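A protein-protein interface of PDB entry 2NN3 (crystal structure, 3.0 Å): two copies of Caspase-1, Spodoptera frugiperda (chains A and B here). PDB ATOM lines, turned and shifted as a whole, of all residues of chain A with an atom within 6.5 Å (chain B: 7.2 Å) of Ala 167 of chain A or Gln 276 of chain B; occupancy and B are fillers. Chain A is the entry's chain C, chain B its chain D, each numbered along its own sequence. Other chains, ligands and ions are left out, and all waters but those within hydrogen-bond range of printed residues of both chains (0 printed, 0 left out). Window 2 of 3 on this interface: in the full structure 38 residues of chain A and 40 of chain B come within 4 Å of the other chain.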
ATOM      1  N   ARG A  48      16.901   9.896  -3.223  1.00  0.00           N
ATOM      2  CA  ARG A  48      15.749  10.656  -2.735  1.00  0.00           C
ATOM      3  C   ARG A  48      15.623  11.922  -3.578  1.00  0.00           C
ATOM      4  O   ARG A  48      14.517  12.486  -3.701  1.00  0.00           O
ATOM      5  CB  ARG A  48      15.911  11.031  -1.256  1.00  0.00           C
ATOM      6  CG  ARG A  48      15.595   9.901  -0.276  1.00  0.00           C
ATOM      7  CD  ARG A  48      14.908  10.409   1.010  1.00  0.00           C
ATOM      8  NE  ARG A  48      13.664  11.158   0.758  1.00  0.00           N
ATOM      9  CZ  ARG A  48      12.547  10.654   0.223  1.00  0.00           C
ATOM     10  NH1 ARG A  48      12.487   9.380  -0.151  1.00  0.00           N
ATOM     11  NH2 ARG A  48      11.481  11.433   0.051  1.00  0.00           N
ATOM     12  N   PHE A 158      -6.325  11.889   0.587  1.00  0.00           N
ATOM     13  CA  PHE A 158      -5.155  11.267  -0.043  1.00  0.00           C
ATOM     14  C   PHE A 158      -3.782  11.669   0.543  1.00  0.00           C
ATOM     15  O   PHE A 158      -2.738  11.129   0.172  1.00  0.00           O
ATOM     16  CB  PHE A 158      -5.235  11.399  -1.562  1.00  0.00           C
ATOM     17  CG  PHE A 158      -6.352  10.578  -2.178  1.00  0.00           C
ATOM     18  CD1 PHE A 158      -6.183   9.220  -2.436  1.00  0.00           C
ATOM     19  CD2 PHE A 158      -7.580  11.163  -2.503  1.00  0.00           C
ATOM     20  CE1 PHE A 158      -7.223   8.465  -3.011  1.00  0.00           C
ATOM     21  CE2 PHE A 158      -8.625  10.403  -3.083  1.00  0.00           C
ATOM     22  CZ  PHE A 158      -8.444   9.064  -3.330  1.00  0.00           C
ATOM     23  N   ALA A 160      -0.493  12.028   2.904  1.00  0.00           N
ATOM     24  CA  ALA A 160       0.398  10.956   3.394  1.00  0.00           C
ATOM     25  C   ALA A 160       0.001  10.371   4.746  1.00  0.00           C
ATOM     26  O   ALA A 160       0.038   9.157   4.936  1.00  0.00           O
ATOM     27  CB  ALA A 160       1.822  11.423   3.428  1.00  0.00           C
ATOM     28  N   CYS A 163      -3.064   8.500   3.601  1.00  0.00           N
ATOM     29  CA  CYS A 163      -2.853   7.485   2.598  1.00  0.00           C
ATOM     30  C   CYS A 163      -1.372   7.167   2.493  1.00  0.00           C
ATOM     31  O   CYS A 163      -0.748   7.443   1.469  1.00  0.00           O
ATOM     32  CB  CYS A 163      -3.437   7.933   1.275  1.00  0.00           C
ATOM     33  SG  CYS A 163      -3.876   6.544   0.283  1.00  0.00           S
ATOM     34  N   PRO A 164      -0.810   6.562   3.561  1.00  0.00           N
ATOM     35  CA  PRO A 164       0.629   6.373   3.685  1.00  0.00           C
ATOM     36  C   PRO A 164       1.150   5.463   2.609  1.00  0.00           C
ATOM     37  O   PRO A 164       2.357   5.431   2.373  1.00  0.00           O
ATOM     38  CB  PRO A 164       0.786   5.698   5.049  1.00  0.00           C
ATOM     39  CG  PRO A 164      -0.460   5.975   5.761  1.00  0.00           C
ATOM     40  CD  PRO A 164      -1.517   5.994   4.719  1.00  0.00           C
ATOM     41  N   THR A 165       0.241   4.741   1.961  1.00  0.00           N
ATOM     42  CA  THR A 165       0.616   3.801   0.918  1.00  0.00           C
ATOM     43  C   THR A 165       0.847   4.492  -0.439  1.00  0.00           C
ATOM     44  O   THR A 165       1.538   3.942  -1.302  1.00  0.00           O
ATOM     45  CB  THR A 165      -0.376   2.611   0.837  1.00  0.00           C
ATOM     46  OG1 THR A 165       0.074   1.665  -0.141  1.00  0.00           O
ATOM     47  CG2 THR A 165      -1.784   3.089   0.501  1.00  0.00           C
ATOM     48  N   LEU A 166       0.285   5.698  -0.600  1.00  0.00           N
ATOM     49  CA  LEU A 166       0.516   6.571  -1.781  1.00  0.00           C
ATOM     50  C   LEU A 166       1.581   7.650  -1.531  1.00  0.00           C
ATOM     51  O   LEU A 166       1.797   8.544  -2.357  1.00  0.00           O
ATOM     52  CB  LEU A 166      -0.784   7.260  -2.208  1.00  0.00           C
ATOM     53  CG  LEU A 166      -1.725   6.453  -3.090  1.00  0.00           C
ATOM     54  CD1 LEU A 166      -3.066   7.148  -3.239  1.00  0.00           C
ATOM     55  CD2 LEU A 166      -1.078   6.212  -4.448  1.00  0.00           C
ATOM     56  N   ALA A 167       2.231   7.561  -0.377  1.00  0.00           N
ATOM     57  CA  ALA A 167       3.260   8.495  -0.007  1.00  0.00           C
ATOM     58  C   ALA A 167       4.312   8.558  -1.121  1.00  0.00           C
ATOM     59  O   ALA A 167       4.802   7.512  -1.569  1.00  0.00           O
ATOM     60  CB  ALA A 167       3.875   8.063   1.294  1.00  0.00           C
ATOM     61  N   GLY A 168       4.615   9.773  -1.594  1.00  0.00           N
ATOM     62  CA  GLY A 168       5.601   9.979  -2.656  1.00  0.00           C
ATOM     63  C   GLY A 168       5.134   9.617  -4.057  1.00  0.00           C
ATOM     64  O   GLY A 168       5.801   9.925  -5.035  1.00  0.00           O
ATOM     65  N   LYS A 169       4.001   8.943  -4.173  1.00  0.00           N
ATOM     66  CA  LYS A 169       3.436   8.677  -5.484  1.00  0.00           C
ATOM     67  C   LYS A 169       2.627   9.906  -5.943  1.00  0.00           C
ATOM     68  O   LYS A 169       1.984  10.593  -5.112  1.00  0.00           O
ATOM     69  CB  LYS A 169       2.557   7.421  -5.436  1.00  0.00           C
ATOM     70  CG  LYS A 169       3.351   6.136  -5.301  1.00  0.00           C
ATOM     71  CD  LYS A 169       2.610   5.057  -4.556  1.00  0.00           C
ATOM     72  CE  LYS A 169       3.647   4.196  -3.910  1.00  0.00           C
ATOM     73  NZ  LYS A 169       3.225   2.787  -3.751  1.00  0.00           N
ATOM     74  N   LYS A 171      -0.363  12.114  -7.134  1.00  0.00           N
ATOM     75  CA  LYS A 171      -1.818  12.030  -7.002  1.00  0.00           C
ATOM     76  C   LYS A 171      -2.436  13.102  -7.900  1.00  0.00           C
ATOM     77  O   LYS A 171      -2.317  14.280  -7.620  1.00  0.00           O
ATOM     78  CB  LYS A 171      -2.234  12.230  -5.548  1.00  0.00           C
ATOM     79  CG  LYS A 171      -1.521  11.333  -4.535  1.00  0.00           C
ATOM     80  CD  LYS A 171      -1.405  12.083  -3.214  1.00  0.00           C
ATOM     81  CE  LYS A 171      -0.393  11.467  -2.230  1.00  0.00           C
ATOM     82  NZ  LYS A 171       1.070  11.689  -2.533  1.00  0.00           N
ATOM     83  N   ASP A 209       3.512  16.323  -4.168  1.00  0.00           N
ATOM     84  CA  ASP A 209       3.086  15.230  -5.037  1.00  0.00           C
ATOM     85  C   ASP A 209       1.627  15.250  -5.380  1.00  0.00           C
ATOM     86  O   ASP A 209       1.099  14.261  -5.881  1.00  0.00           O
ATOM     87  CB  ASP A 209       3.459  13.868  -4.457  1.00  0.00           C
ATOM     88  CG  ASP A 209       4.919  13.767  -4.125  1.00  0.00           C
ATOM     89  OD1 ASP A 209       5.766  14.137  -4.970  1.00  0.00           O
ATOM     90  OD2 ASP A 209       5.215  13.324  -3.002  1.00  0.00           O
ATOM     91  N   ALA B 261      10.764  20.198  -0.205  1.00  0.00           N
ATOM     92  CA  ALA B 261      10.189  19.032   0.405  1.00  0.00           C
ATOM     93  C   ALA B 261      11.251  18.344   1.229  1.00  0.00           C
ATOM     94  O   ALA B 261      10.950  17.862   2.320  1.00  0.00           O
ATOM     95  CB  ALA B 261       9.658  18.114  -0.628  1.00  0.00           C
ATOM     96  N   LEU B 262      12.498  18.330   0.731  1.00  0.00           N
ATOM     97  CA  LEU B 262      13.583  17.539   1.354  1.00  0.00           C
ATOM     98  C   LEU B 262      14.144  18.088   2.665  1.00  0.00           C
ATOM     99  O   LEU B 262      14.603  17.326   3.503  1.00  0.00           O
ATOM    100  CB  LEU B 262      14.717  17.230   0.360  1.00  0.00           C
ATOM    101  CG  LEU B 262      14.597  15.903  -0.424  1.00  0.00           C
ATOM    102  CD1 LEU B 262      15.449  15.917  -1.707  1.00  0.00           C
ATOM    103  CD2 LEU B 262      14.921  14.643   0.449  1.00  0.00           C
ATOM    104  N   PHE B 264      12.221  19.848   4.714  1.00  0.00           N
ATOM    105  CA  PHE B 264      11.071  19.460   5.489  1.00  0.00           C
ATOM    106  C   PHE B 264      11.218  18.001   6.005  1.00  0.00           C
ATOM    107  O   PHE B 264      10.940  17.000   5.318  1.00  0.00           O
ATOM    108  CB  PHE B 264       9.854  19.678   4.615  1.00  0.00           C
ATOM    109  CG  PHE B 264       8.582  19.683   5.367  1.00  0.00           C
ATOM    110  CD1 PHE B 264       7.830  18.528   5.484  1.00  0.00           C
ATOM    111  CD2 PHE B 264       8.145  20.829   5.995  1.00  0.00           C
ATOM    112  CE1 PHE B 264       6.675  18.518   6.193  1.00  0.00           C
ATOM    113  CE2 PHE B 264       6.970  20.808   6.712  1.00  0.00           C
ATOM    114  CZ  PHE B 264       6.244  19.651   6.810  1.00  0.00           C
ATOM    115  N   ASP B 270       7.441  14.688  13.117  1.00  0.00           N
ATOM    116  CA  ASP B 270       8.093  13.674  12.250  1.00  0.00           C
ATOM    117  C   ASP B 270       9.339  12.993  12.875  1.00  0.00           C
ATOM    118  O   ASP B 270      10.333  12.741  12.182  1.00  0.00           O
ATOM    119  CB  ASP B 270       8.456  14.296  10.881  1.00  0.00           C
ATOM    120  CG  ASP B 270       7.235  14.810  10.108  1.00  0.00           C
ATOM    121  OD1 ASP B 270       6.425  13.977   9.639  1.00  0.00           O
ATOM    122  OD2 ASP B 270       7.099  16.048   9.947  1.00  0.00           O
ATOM    123  N   MET B 274      12.252   7.521   7.629  1.00  0.00           N
ATOM    124  CA  MET B 274      12.401   8.124   6.310  1.00  0.00           C
ATOM    125  C   MET B 274      11.216   9.051   6.030  1.00  0.00           C
ATOM    126  O   MET B 274      11.389  10.171   5.512  1.00  0.00           O
ATOM    127  CB  MET B 274      12.443   7.042   5.214  1.00  0.00           C
ATOM    128  CG  MET B 274      12.575   5.588   5.691  1.00  0.00           C
ATOM    129  SD  MET B 274      14.242   4.876   5.600  1.00  0.00           S
ATOM    130  CE  MET B 274      15.089   5.652   6.991  1.00  0.00           C
ATOM    131  N   HIS B 275      10.019   8.558   6.376  1.00  0.00           N
ATOM    132  CA  HIS B 275       8.728   9.168   6.010  1.00  0.00           C
ATOM    133  C   HIS B 275       8.425   9.039   4.503  1.00  0.00           C
ATOM    134  O   HIS B 275       9.006   8.207   3.800  1.00  0.00           O
ATOM    135  CB  HIS B 275       8.652  10.645   6.474  1.00  0.00           C
ATOM    136  N   GLN B 276       7.485   9.847   4.025  1.00  0.00           N
ATOM    137  CA  GLN B 276       7.276  10.024   2.598  1.00  0.00           C
ATOM    138  C   GLN B 276       7.844  11.393   2.192  1.00  0.00           C
ATOM    139  O   GLN B 276       9.081  11.585   2.186  1.00  0.00           O
ATOM    140  CB  GLN B 276       5.813   9.928   2.272  1.00  0.00           C
ATOM    141  N   GLN B 277       6.951  12.350   1.900  1.00  0.00           N
ATOM    142  CA  GLN B 277       7.387  13.649   1.363  1.00  0.00           C
ATOM    143  C   GLN B 277       7.255  14.886   2.283  1.00  0.00           C
ATOM    144  O   GLN B 277       7.974  14.944   3.289  1.00  0.00           O
ATOM    145  CB  GLN B 277       6.842  13.850  -0.062  1.00  0.00           C
ATOM    146  CG  GLN B 277       7.605  13.023  -1.120  1.00  0.00           C
ATOM    147  CD  GLN B 277       8.916  13.677  -1.593  1.00  0.00           C
ATOM    148  OE1 GLN B 277       9.656  14.294  -0.811  1.00  0.00           O
ATOM    149  NE2 GLN B 277       9.206  13.529  -2.885  1.00  0.00           N
ATOM    150  N   LYS B 278       6.370  15.855   1.967  1.00  0.00           N
ATOM    151  CA  LYS B 278       6.344  17.130   2.727  1.00  0.00           C
ATOM    152  C   LYS B 278       5.240  18.204   2.496  1.00  0.00           C
ATOM    153  O   LYS B 278       4.068  17.892   2.237  1.00  0.00           O
ATOM    154  CB  LYS B 278       7.700  17.793   2.589  1.00  0.00           C
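O of Gln 276 of chain B sits at hydrogen-bond distance from NH2 of Arg 48 of chain A, at 3.2 Å.
O of Asp 209 of chain A lies within hydrogen-bond range of N of Lys 171 of chain A, 2.9 Å away.
Among the printed residues, pairs that only touch across the chains: Arg 48 of chain A with Leu 262 of chain B (3.7 Å), Arg 48 of chain A with Gln 277 of chain B (3.5 Å), Ala 167 of chain A with Gln 276 of chain B (2.9 Å), Gly 168 of chain A with Gln 277 of chain B (3.95 Å) and Asp 209 of chain A with Gln 277 of chain B (3.1 Å).
Ala 167 of chain A touches just one residue of chain B: Gln 276. Of the printed residues of chain A, Leu 262 of chain B touches Arg 48 (3.7 Å). Of the printed residues of chain B, Arg 48 of chain A touches Leu 262, Gln 276 and Gln 277. His 275 of chain B touches none of the printed residues of chain A. Ala 261 of chain B touches none of the printed residues of chain A. The nearest residue of chain A that does not touch Gln 276 of chain B is Gly 168 of chain A (4.1 Å). The nearest printed residue of chain B that does not touch Arg 48 of chain A is Met 274 of chain B (5.4 Å).
Hydrophobic or aromatic side chains of chain A that line the printed part of chain B: Ala 167. Along chain A the printed residues that touch a printed residue of chain B span positions 48 to 209. Among the printed residues, 6 pairs touch across the chains. Among the printed residues, no Asp or Glu carboxylate lies within 4 Å of a Lys or Arg side-chain nitrogen of the other chain.
No position is printed for both chains. Of the 6 pairs that touch across the chains among the printed residues, none has its exchanged pair printed and touching as well.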
